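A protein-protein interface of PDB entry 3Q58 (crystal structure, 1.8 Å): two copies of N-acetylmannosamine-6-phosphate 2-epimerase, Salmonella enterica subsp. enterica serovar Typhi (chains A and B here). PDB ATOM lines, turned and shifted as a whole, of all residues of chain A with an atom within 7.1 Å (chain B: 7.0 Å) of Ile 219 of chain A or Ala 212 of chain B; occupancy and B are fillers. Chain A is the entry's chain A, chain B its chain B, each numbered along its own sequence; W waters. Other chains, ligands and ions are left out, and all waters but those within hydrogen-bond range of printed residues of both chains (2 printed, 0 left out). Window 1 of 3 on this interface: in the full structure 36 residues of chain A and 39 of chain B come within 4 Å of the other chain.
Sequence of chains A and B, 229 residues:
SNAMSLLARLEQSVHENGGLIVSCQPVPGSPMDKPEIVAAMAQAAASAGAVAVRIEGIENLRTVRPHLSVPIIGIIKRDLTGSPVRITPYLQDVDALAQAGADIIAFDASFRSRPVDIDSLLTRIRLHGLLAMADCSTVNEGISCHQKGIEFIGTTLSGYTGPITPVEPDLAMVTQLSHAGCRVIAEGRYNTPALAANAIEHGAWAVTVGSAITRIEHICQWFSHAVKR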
ATOM      1  N   GLY A 210      10.736  21.219 -27.427  1.00  0.00           N
ATOM      2  CA  GLY A 210      10.643  20.487 -26.180  1.00  0.00           C
ATOM      3  C   GLY A 210       9.257  19.926 -25.922  1.00  0.00           C
ATOM      4  O   GLY A 210       8.971  18.780 -26.258  1.00  0.00           O
ATOM      5  N   SER A 211       8.396  20.745 -25.331  1.00  0.00           N
ATOM      6  CA  SER A 211       7.071  20.307 -24.890  1.00  0.00           C
ATOM      7  C   SER A 211       6.255  19.543 -25.939  1.00  0.00           C
ATOM      8  O   SER A 211       5.672  18.504 -25.638  1.00  0.00           O
ATOM      9  CB  SER A 211       6.264  21.502 -24.382  1.00  0.00           C
ATOM     10  OG  SER A 211       6.958  22.143 -23.326  1.00  0.00           O
ATOM     11  N   ALA A 212       6.221  20.063 -27.161  1.00  0.00           N
ATOM     12  CA  ALA A 212       5.390  19.490 -28.221  1.00  0.00           C
ATOM     13  C   ALA A 212       5.811  18.066 -28.560  1.00  0.00           C
ATOM     14  O   ALA A 212       5.080  17.340 -29.235  1.00  0.00           O
ATOM     15  CB  ALA A 212       5.443  20.359 -29.459  1.00  0.00           C
ATOM     16  N   ILE A 213       6.987  17.660 -28.093  1.00  0.00           N
ATOM     17  CA  ILE A 213       7.468  16.316 -28.393  1.00  0.00           C
ATOM     18  C   ILE A 213       7.600  15.434 -27.151  1.00  0.00           C
ATOM     19  O   ILE A 213       7.282  14.246 -27.198  1.00  0.00           O
ATOM     20  CB  ILE A 213       8.812  16.346 -29.172  1.00  0.00           C
ATOM     21  CG1 ILE A 213       8.649  17.078 -30.509  1.00  0.00           C
ATOM     22  CG2 ILE A 213       9.333  14.921 -29.400  1.00  0.00           C
ATOM     23  CD1 ILE A 213       9.980  17.354 -31.233  1.00  0.00           C
ATOM     24  N   THR A 214       8.044  16.005 -26.034  1.00  0.00           N
ATOM     25  CA  THR A 214       8.389  15.174 -24.880  1.00  0.00           C
ATOM     26  C   THR A 214       7.657  15.514 -23.577  1.00  0.00           C
ATOM     27  O   THR A 214       8.000  14.992 -22.511  1.00  0.00           O
ATOM     28  CB  THR A 214       9.894  15.210 -24.628  1.00  0.00           C
ATOM     29  OG1 THR A 214      10.298  16.572 -24.425  1.00  0.00           O
ATOM     30  CG2 THR A 214      10.654  14.622 -25.840  1.00  0.00           C
ATOM     31  N   ARG A 215       6.663  16.392 -23.641  1.00  0.00           N
ATOM     32  CA  ARG A 215       5.851  16.647 -22.451  1.00  0.00           C
ATOM     33  C   ARG A 215       4.388  16.299 -22.685  1.00  0.00           C
ATOM     34  O   ARG A 215       3.585  17.157 -23.044  1.00  0.00           O
ATOM     35  CB  ARG A 215       5.983  18.102 -21.971  1.00  0.00           C
ATOM     36  CG  ARG A 215       7.241  18.373 -21.147  1.00  0.00           C
ATOM     37  CD  ARG A 215       7.216  19.768 -20.515  1.00  0.00           C
ATOM     38  NE  ARG A 215       8.450  20.054 -19.780  1.00  0.00           N
ATOM     39  CZ  ARG A 215       9.234  21.101 -20.012  1.00  0.00           C
ATOM     40  NH1 ARG A 215       8.914  21.978 -20.953  1.00  0.00           N
ATOM     41  NH2 ARG A 215      10.338  21.276 -19.297  1.00  0.00           N
ATOM     42  N   ILE A 216       4.046  15.032 -22.481  1.00  0.00           N
ATOM     43  CA  ILE A 216       2.680  14.570 -22.728  1.00  0.00           C
ATOM     44  C   ILE A 216       1.616  15.409 -22.018  1.00  0.00           C
ATOM     45  O   ILE A 216       0.608  15.773 -22.624  1.00  0.00           O
ATOM     46  CB  ILE A 216       2.530  13.065 -22.404  1.00  0.00           C
ATOM     47  CG1 ILE A 216       3.303  12.256 -23.450  1.00  0.00           C
ATOM     48  CG2 ILE A 216       1.052  12.656 -22.388  1.00  0.00           C
ATOM     49  CD1 ILE A 216       3.152  10.754 -23.314  1.00  0.00           C
ATOM     50  N   GLU A 217       1.842  15.737 -20.747  1.00  0.00           N
ATOM     51  CA  GLU A 217       0.863  16.517 -19.992  1.00  0.00           C
ATOM     52  C   GLU A 217       0.550  17.852 -20.656  1.00  0.00           C
ATOM     53  O   GLU A 217      -0.599  18.289 -20.675  1.00  0.00           O
ATOM     54  CB  GLU A 217       1.339  16.771 -18.564  1.00  0.00           C
ATOM     55  CG  GLU A 217       1.398  15.530 -17.721  1.00  0.00           C
ATOM     56  CD  GLU A 217       2.747  14.867 -17.767  1.00  0.00           C
ATOM     57  OE1 GLU A 217       3.517  15.130 -18.720  1.00  0.00           O
ATOM     58  OE2 GLU A 217       3.045  14.095 -16.831  1.00  0.00           O
ATOM     59  N   HIS A 218       1.577  18.510 -21.179  1.00  0.00           N
ATOM     60  CA  HIS A 218       1.376  19.793 -21.840  1.00  0.00           C
ATOM     61  C   HIS A 218       0.631  19.652 -23.166  1.00  0.00           C
ATOM     62  O   HIS A 218      -0.247  20.459 -23.472  1.00  0.00           O
ATOM     63  CB  HIS A 218       2.714  20.513 -22.050  1.00  0.00           C
ATOM     64  CG  HIS A 218       3.287  21.071 -20.787  1.00  0.00           C
ATOM     65  ND1 HIS A 218       4.302  22.005 -20.773  1.00  0.00           N
ATOM     66  CD2 HIS A 218       2.978  20.835 -19.490  1.00  0.00           C
ATOM     67  CE1 HIS A 218       4.597  22.312 -19.521  1.00  0.00           C
ATOM     68  NE2 HIS A 218       3.806  21.615 -18.722  1.00  0.00           N
ATOM     69  N   ILE A 219       0.992  18.647 -23.956  1.00  0.00           N
ATOM     70  CA  ILE A 219       0.316  18.430 -25.238  1.00  0.00           C
ATOM     71  C   ILE A 219      -1.165  18.138 -24.980  1.00  0.00           C
ATOM     72  O   ILE A 219      -2.049  18.709 -25.632  1.00  0.00           O
ATOM     73  CB  ILE A 219       0.966  17.287 -26.063  1.00  0.00           C
ATOM     74  CG1 ILE A 219       2.470  17.513 -26.233  1.00  0.00           C
ATOM     75  CG2 ILE A 219       0.286  17.143 -27.438  1.00  0.00           C
ATOM     76  CD1 ILE A 219       3.206  16.286 -26.737  1.00  0.00           C
ATOM     77  N   CYS A 220      -1.444  17.277 -24.005  1.00  0.00           N
ATOM     78  CA  CYS A 220      -2.831  16.973 -23.646  1.00  0.00           C
ATOM     79  C   CYS A 220      -3.619  18.210 -23.243  1.00  0.00           C
ATOM     80  O   CYS A 220      -4.790  18.346 -23.598  1.00  0.00           O
ATOM     81  CB  CYS A 220      -2.899  15.948 -22.518  1.00  0.00           C
ATOM     82  SG  CYS A 220      -2.421  14.300 -23.014  1.00  0.00           S
ATOM     83  N   GLN A 221      -2.989  19.087 -22.468  1.00  0.00           N
ATOM     84  CA  GLN A 221      -3.619  20.335 -22.055  1.00  0.00           C
ATOM     85  C   GLN A 221      -4.027  21.164 -23.273  1.00  0.00           C
ATOM     86  O   GLN A 221      -5.106  21.758 -23.285  1.00  0.00           O
ATOM     87  CB  GLN A 221      -2.680  21.153 -21.148  1.00  0.00           C
ATOM     88  CG  GLN A 221      -2.474  20.571 -19.747  1.00  0.00           C
ATOM     89  CD  GLN A 221      -1.299  21.215 -18.985  1.00  0.00           C
ATOM     90  OE1 GLN A 221      -0.599  22.095 -19.502  1.00  0.00           O
ATOM     91  NE2 GLN A 221      -1.085  20.768 -17.748  1.00  0.00           N
ATOM     92  N   TRP A 222      -3.159  21.208 -24.288  1.00  0.00           N
ATOM     93  CA  TRP A 222      -3.444  21.966 -25.509  1.00  0.00           C
ATOM     94  C   TRP A 222      -4.685  21.425 -26.209  1.00  0.00           C
ATOM     95  O   TRP A 222      -5.554  22.185 -26.636  1.00  0.00           O
ATOM     96  CB  TRP A 222      -2.265  21.914 -26.480  1.00  0.00           C
ATOM     97  CG  TRP A 222      -0.972  22.441 -25.900  1.00  0.00           C
ATOM     98  CD1 TRP A 222      -0.832  23.268 -24.818  1.00  0.00           C
ATOM     99  CD2 TRP A 222       0.353  22.159 -26.363  1.00  0.00           C
ATOM    100  NE1 TRP A 222       0.507  23.523 -24.583  1.00  0.00           N
ATOM    101  CE2 TRP A 222       1.252  22.852 -25.520  1.00  0.00           C
ATOM    102  CE3 TRP A 222       0.870  21.388 -27.414  1.00  0.00           C
ATOM    103  CZ2 TRP A 222       2.635  22.792 -25.695  1.00  0.00           C
ATOM    104  CZ3 TRP A 222       2.241  21.334 -27.585  1.00  0.00           C
ATOM    105  CH2 TRP A 222       3.106  22.032 -26.733  1.00  0.00           C
ATOM    106  N   PHE A 223      -4.754  20.105 -26.342  1.00  0.00           N
ATOM    107  CA  PHE A 223      -5.908  19.476 -26.967  1.00  0.00           C
ATOM    108  C   PHE A 223      -7.147  19.579 -26.079  1.00  0.00           C
ATOM    109  O   PHE A 223      -8.241  19.857 -26.564  1.00  0.00           O
ATOM    110  CB  PHE A 223      -5.601  18.010 -27.329  1.00  0.00           C
ATOM    111  CG  PHE A 223      -4.762  17.853 -28.575  1.00  0.00           C
ATOM    112  CD1 PHE A 223      -5.362  17.701 -29.819  1.00  0.00           C
ATOM    113  CD2 PHE A 223      -3.377  17.865 -28.502  1.00  0.00           C
ATOM    114  CE1 PHE A 223      -4.600  17.562 -30.964  1.00  0.00           C
ATOM    115  CE2 PHE A 223      -2.601  17.730 -29.640  1.00  0.00           C
ATOM    116  CZ  PHE A 223      -3.208  17.578 -30.877  1.00  0.00           C
ATOM    117  N   SER A 224      -7.001  19.372 -24.803  1.00  0.00           N
ATOM    118  CA  SER A 224      -8.113  19.441 -23.889  1.00  0.00           C
ATOM    119  C   SER A 224      -8.721  20.815 -23.921  1.00  0.00           C
ATOM    120  O   SER A 224      -9.890  20.982 -24.057  1.00  0.00           O
ATOM    121  CB  SER A 224      -7.633  19.092 -22.514  1.00  0.00           C
ATOM    122  OG  SER A 224      -8.571  19.371 -21.554  1.00  0.00           O
ATOM    123  N   HIS A 225      -7.907  21.818 -23.931  1.00  0.00           N
ATOM    124  CA  HIS A 225      -8.424  23.122 -24.035  1.00  0.00           C
ATOM    125  C   HIS A 225      -9.203  23.360 -25.319  1.00  0.00           C
ATOM    126  O   HIS A 225     -10.184  24.030 -25.301  1.00  0.00           O
ATOM    127  CB  HIS A 225      -7.275  24.082 -23.981  1.00  0.00           C
ATOM    128  CG  HIS A 225      -7.672  25.495 -24.127  1.00  0.00           C
ATOM    129  ND1 HIS A 225      -7.972  26.294 -23.051  1.00  0.00           N
ATOM    130  CD2 HIS A 225      -7.792  26.273 -25.224  1.00  0.00           C
ATOM    131  CE1 HIS A 225      -8.258  27.505 -23.481  1.00  0.00           C
ATOM    132  NE2 HIS A 225      -8.154  27.517 -24.795  1.00  0.00           N
ATOM    133  N   LEU B  20     -11.668  14.687 -24.679  1.00  0.00           N
ATOM    134  CA  LEU B  20     -10.379  14.268 -25.198  1.00  0.00           C
ATOM    135  C   LEU B  20     -10.076  12.844 -24.769  1.00  0.00           C
ATOM    136  O   LEU B  20     -10.042  12.532 -23.577  1.00  0.00           O
ATOM    137  CB  LEU B  20      -9.255  15.191 -24.719  1.00  0.00           C
ATOM    138  CG  LEU B  20      -7.841  14.698 -25.047  1.00  0.00           C
ATOM    139  CD1 LEU B  20      -7.547  14.733 -26.548  1.00  0.00           C
ATOM    140  CD2 LEU B  20      -6.775  15.493 -24.264  1.00  0.00           C
ATOM    141  N   ALA B  48      -3.930  14.895 -17.237  1.00  0.00           N
ATOM    142  CA  ALA B  48      -3.848  16.178 -17.934  1.00  0.00           C
ATOM    143  C   ALA B  48      -4.977  16.452 -18.921  1.00  0.00           C
ATOM    144  O   ALA B  48      -4.814  17.262 -19.835  1.00  0.00           O
ATOM    145  CB  ALA B  48      -2.497  16.306 -18.643  1.00  0.00           C
ATOM    146  N   TYR B 190      -6.542  13.795 -36.255  1.00  0.00           N
ATOM    147  CA  TYR B 190      -6.784  14.982 -35.444  1.00  0.00           C
ATOM    148  C   TYR B 190      -5.516  15.328 -34.675  1.00  0.00           C
ATOM    149  O   TYR B 190      -5.443  15.170 -33.459  1.00  0.00           O
ATOM    150  CB  TYR B 190      -7.980  14.780 -34.517  1.00  0.00           C
ATOM    151  CG  TYR B 190      -9.269  14.658 -35.311  1.00  0.00           C
ATOM    152  CD1 TYR B 190      -9.911  15.797 -35.797  1.00  0.00           C
ATOM    153  CD2 TYR B 190      -9.805  13.414 -35.620  1.00  0.00           C
ATOM    154  CE1 TYR B 190     -11.068  15.709 -36.551  1.00  0.00           C
ATOM    155  CE2 TYR B 190     -10.981  13.310 -36.378  1.00  0.00           C
ATOM    156  CZ  TYR B 190     -11.597  14.468 -36.841  1.00  0.00           C
ATOM    157  OH  TYR B 190     -12.753  14.399 -37.588  1.00  0.00           O
ATOM    158  N   ASN B 191      -4.511  15.793 -35.407  1.00  0.00           N
ATOM    159  CA  ASN B 191      -3.179  15.983 -34.841  1.00  0.00           C
ATOM    160  C   ASN B 191      -2.769  17.428 -34.580  1.00  0.00           C
ATOM    161  O   ASN B 191      -1.595  17.708 -34.317  1.00  0.00           O
ATOM    162  CB  ASN B 191      -2.140  15.286 -35.707  1.00  0.00           C
ATOM    163  CG  ASN B 191      -2.234  13.790 -35.597  1.00  0.00           C
ATOM    164  OD1 ASN B 191      -2.405  13.252 -34.490  1.00  0.00           O
ATOM    165  ND2 ASN B 191      -2.170  13.104 -36.738  1.00  0.00           N
ATOM    166  N   THR B 192      -3.730  18.336 -34.656  1.00  0.00           N
ATOM    167  CA  THR B 192      -3.543  19.667 -34.091  1.00  0.00           C
ATOM    168  C   THR B 192      -4.732  19.982 -33.199  1.00  0.00           C
ATOM    169  O   THR B 192      -5.823  19.452 -33.404  1.00  0.00           O
ATOM    170  CB  THR B 192      -3.431  20.739 -35.166  1.00  0.00           C
ATOM    171  OG1 THR B 192      -4.712  20.936 -35.771  1.00  0.00           O
ATOM    172  CG2 THR B 192      -2.406  20.325 -36.216  1.00  0.00           C
ATOM    173  N   PRO B 193      -4.523  20.821 -32.178  1.00  0.00           N
ATOM    174  CA  PRO B 193      -5.655  21.212 -31.337  1.00  0.00           C
ATOM    175  C   PRO B 193      -6.775  21.846 -32.162  1.00  0.00           C
ATOM    176  O   PRO B 193      -7.950  21.649 -31.856  1.00  0.00           O
ATOM    177  CB  PRO B 193      -5.033  22.247 -30.393  1.00  0.00           C
ATOM    178  CG  PRO B 193      -3.598  21.800 -30.269  1.00  0.00           C
ATOM    179  CD  PRO B 193      -3.227  21.300 -31.641  1.00  0.00           C
ATOM    180  N   VAL B 209      -7.066  11.436 -29.924  1.00  0.00           N
ATOM    181  CA  VAL B 209      -5.789  11.861 -30.474  1.00  0.00           C
ATOM    182  C   VAL B 209      -4.722  10.838 -30.106  1.00  0.00           C
ATOM    183  O   VAL B 209      -4.626  10.423 -28.952  1.00  0.00           O
ATOM    184  CB  VAL B 209      -5.379  13.229 -29.918  1.00  0.00           C
ATOM    185  CG1 VAL B 209      -4.038  13.690 -30.531  1.00  0.00           C
ATOM    186  CG2 VAL B 209      -6.477  14.248 -30.189  1.00  0.00           C
ATOM    187  N   GLY B 210      -3.941  10.419 -31.095  1.00  0.00           N
ATOM    188  CA  GLY B 210      -2.886   9.443 -30.883  1.00  0.00           C
ATOM    189  C   GLY B 210      -1.498   9.962 -31.233  1.00  0.00           C
ATOM    190  O   GLY B 210      -0.749  10.374 -30.351  1.00  0.00           O
ATOM    191  N   SER B 211      -1.151   9.939 -32.518  1.00  0.00           N
ATOM    192  CA  SER B 211       0.214  10.254 -32.929  1.00  0.00           C
ATOM    193  C   SER B 211       0.744  11.563 -32.331  1.00  0.00           C
ATOM    194  O   SER B 211       1.869  11.601 -31.852  1.00  0.00           O
ATOM    195  CB  SER B 211       0.346  10.264 -34.456  1.00  0.00           C
ATOM    196  OG  SER B 211      -0.047   9.013 -35.006  1.00  0.00           O
ATOM    197  N   ALA B 212      -0.063  12.622 -32.338  1.00  0.00           N
ATOM    198  CA  ALA B 212       0.436  13.936 -31.909  1.00  0.00           C
ATOM    199  C   ALA B 212       0.801  13.985 -30.424  1.00  0.00           C
ATOM    200  O   ALA B 212       1.431  14.945 -29.963  1.00  0.00           O
ATOM    201  CB  ALA B 212      -0.584  15.033 -32.233  1.00  0.00           C
ATOM    202  N   ILE B 213       0.386  12.966 -29.676  1.00  0.00           N
ATOM    203  CA  ILE B 213       0.635  12.920 -28.241  1.00  0.00           C
ATOM    204  C   ILE B 213       1.608  11.796 -27.871  1.00  0.00           C
ATOM    205  O   ILE B 213       2.496  11.993 -27.036  1.00  0.00           O
ATOM    206  CB  ILE B 213      -0.686  12.776 -27.439  1.00  0.00           C
ATOM    207  CG1 ILE B 213      -1.616  13.967 -27.711  1.00  0.00           C
ATOM    208  CG2 ILE B 213      -0.413  12.672 -25.931  1.00  0.00           C
ATOM    209  CD1 ILE B 213      -2.999  13.835 -27.050  1.00  0.00           C
ATOM    210  N   THR B 214       1.463  10.638 -28.513  1.00  0.00           N
ATOM    211  CA  THR B 214       2.190   9.439 -28.085  1.00  0.00           C
ATOM    212  C   THR B 214       3.097   8.756 -29.122  1.00  0.00           C
ATOM    213  O   THR B 214       3.590   7.651 -28.873  1.00  0.00           O
ATOM    214  CB  THR B 214       1.206   8.374 -27.572  1.00  0.00           C
ATOM    215  OG1 THR B 214       0.311   8.022 -28.631  1.00  0.00           O
ATOM    216  CG2 THR B 214       0.400   8.912 -26.392  1.00  0.00           C
ATOM    217  N   ARG B 215       3.302   9.369 -30.285  1.00  0.00           N
ATOM    218  CA  ARG B 215       4.228   8.794 -31.261  1.00  0.00           C
ATOM    219  C   ARG B 215       5.360   9.772 -31.553  1.00  0.00           C
ATOM    220  O   ARG B 215       5.290  10.536 -32.512  1.00  0.00           O
ATOM    221  CB  ARG B 215       3.512   8.388 -32.559  1.00  0.00           C
ATOM    222  CG  ARG B 215       2.675   7.125 -32.441  1.00  0.00           C
ATOM    223  CD  ARG B 215       2.306   6.587 -33.818  1.00  0.00           C
ATOM    224  NE  ARG B 215       1.544   5.343 -33.741  1.00  0.00           N
ATOM    225  CZ  ARG B 215       0.266   5.237 -34.084  1.00  0.00           C
ATOM    226  NH1 ARG B 215      -0.383   6.302 -34.536  1.00  0.00           N
ATOM    227  NH2 ARG B 215      -0.359   4.070 -33.985  1.00  0.00           N
ATOM    228  N   HIS B 218       6.702  10.154 -35.077  1.00  0.00           N
ATOM    229  CA  HIS B 218       5.852  10.877 -36.018  1.00  0.00           C
ATOM    230  C   HIS B 218       5.992  12.379 -35.793  1.00  0.00           C
ATOM    231  O   HIS B 218       6.118  13.151 -36.743  1.00  0.00           O
ATOM    232  CB  HIS B 218       4.381  10.448 -35.907  1.00  0.00           C
ATOM    233  CG  HIS B 218       4.113   9.077 -36.447  1.00  0.00           C
ATOM    234  ND1 HIS B 218       2.896   8.714 -36.985  1.00  0.00           N
ATOM    235  CD2 HIS B 218       4.907   7.985 -36.541  1.00  0.00           C
ATOM    236  CE1 HIS B 218       2.953   7.456 -37.383  1.00  0.00           C
ATOM    237  NE2 HIS B 218       4.161   6.989 -37.124  1.00  0.00           N
ATOM    238  N   ILE B 219       5.950  12.789 -34.536  1.00  0.00           N
ATOM    239  CA  ILE B 219       6.003  14.211 -34.235  1.00  0.00           C
ATOM    240  C   ILE B 219       7.326  14.792 -34.705  1.00  0.00           C
ATOM    241  O   ILE B 219       7.373  15.870 -35.303  1.00  0.00           O
ATOM    242  CB  ILE B 219       5.837  14.493 -32.749  1.00  0.00           C
ATOM    243  CG1 ILE B 219       4.566  13.824 -32.208  1.00  0.00           C
ATOM    244  CG2 ILE B 219       5.771  15.983 -32.527  1.00  0.00           C
ATOM    245  CD1 ILE B 219       4.533  13.809 -30.676  1.00  0.00           C
ATOM    246  N   TRP B 222       7.278  15.423 -38.396  1.00  0.00           N
ATOM    247  CA  TRP B 222       6.538  16.620 -38.784  1.00  0.00           C
ATOM    248  C   TRP B 222       7.417  17.857 -38.627  1.00  0.00           C
ATOM    249  O   TRP B 222       7.454  18.718 -39.510  1.00  0.00           O
ATOM    250  CB  TRP B 222       5.258  16.786 -37.963  1.00  0.00           C
ATOM    251  CG  TRP B 222       4.328  15.620 -37.976  1.00  0.00           C
ATOM    252  CD1 TRP B 222       4.221  14.643 -38.930  1.00  0.00           C
ATOM    253  CD2 TRP B 222       3.361  15.314 -36.975  1.00  0.00           C
ATOM    254  NE1 TRP B 222       3.235  13.744 -38.577  1.00  0.00           N
ATOM    255  CE2 TRP B 222       2.695  14.136 -37.379  1.00  0.00           C
ATOM    256  CE3 TRP B 222       2.991  15.923 -35.770  1.00  0.00           C
ATOM    257  CZ2 TRP B 222       1.682  13.557 -36.620  1.00  0.00           C
ATOM    258  CZ3 TRP B 222       1.980  15.345 -35.018  1.00  0.00           C
ATOM    259  CH2 TRP B 222       1.341  14.170 -35.445  1.00  0.00           C
HETATM  260  O   HOH W   1       5.328  12.117 -26.680  1.00  0.00           O
HETATM  261  O   HOH W   2       2.628  17.218 -30.457  1.00  0.00           O
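O of Ile 216 of chain A lies within hydrogen-bond range of SG of Cys 220 of chain A. The indole nitrogen (NE1) of Trp 222 of chain A lies close to the backbone carbonyl oxygen (O) of His 218 of chain A, 3.3 Å away. The backbone NH (N) of Ala 212 of chain B is in hydrogen-bond range of the side-chain amide oxygen (OD1) of Asn 191 of chain B (3.2 Å).
CG1 of Ile 213 of chain A touches CG2 of Ile 219 of chain B, 3.7 Å away. CB of Ala 48 of chain B touches O of Glu 217 of chain A (3.4 Å). Ile 219 of chain A touches Ala 212 of chain B. Cys 220 of chain A touches Ala 48 of chain B. O of Ala 48 of chain B touches N of Gln 221 of chain A (3.7 Å). Phe 223 of chain A touches Leu 20 of chain B. C of Asn 191 of chain B touches CZ of Phe 223 of chain A (3.7 Å). Phe 223 of chain A touches Pro 193 of chain B (CE1 to N, 3.5 Å). Val 209 of chain B touches Phe 223 of chain A. N of Ser 224 of chain A touches CD2 of Leu 20 of chain B (3.9 Å).
Printed residues of chain B within 4 Å of Ile 219 of chain A: Ala 212 and Ile 213. Of the printed residues of chain B, Ser 224 of chain A touches Leu 20 (3.9 Å). Printed residues of chain A within 4 Å of Ala 48 of chain B: Glu 217 (3.4 Å), Cys 220 (3.5 Å) and Gln 221 (3.7 Å). Printed residues of chain A within 4 Å of Ala 212 of chain B: Ile 219 (3.5 Å) and Phe 223 (3.9 Å). The nearest residue of chain B that does not touch Ile 219 of chain A is Ile 219 of chain B (4.8 Å). The nearest residue of chain A that does not touch Ala 212 of chain B is Ala 212 of chain A (4.4 Å).
Printed residues of chain B that touch a printed residue of chain A: Leu 20, Ala 48, Tyr 190, Asn 191, Thr 192, Pro 193, Val 209, Ala 212, Ile 213 and Ile 219. Hydrophobic or aromatic side chains of chain A that line the printed part of chain B: Ile 213, Ile 216, Ile 219 and Phe 223. Among the printed residues, no Asp or Glu carboxylate lies within 4 Å of a Lys or Arg side-chain nitrogen of the other chain.
Ala 212 of chain A touches Ile 219 of chain B, and with the chains exchanged Ile 219 of chain A touches Ala 212 of chain B. Ile 213 of chain A touches Ile 219 of chain B, and with the chains exchanged Ile 219 of chain A touches Ile 213 of chain B.
Water W2 lies within hydrogen-bond range of O of Ala 212 of chain B and O of Ala 212 of chain A. Water W1 lies within hydrogen-bond range of the backbone carbonyl oxygen of Ile 213 of chain B (2.9 Å) and the backbone carbonyl oxygen of Ile 213 of chain A (2.9 Å).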
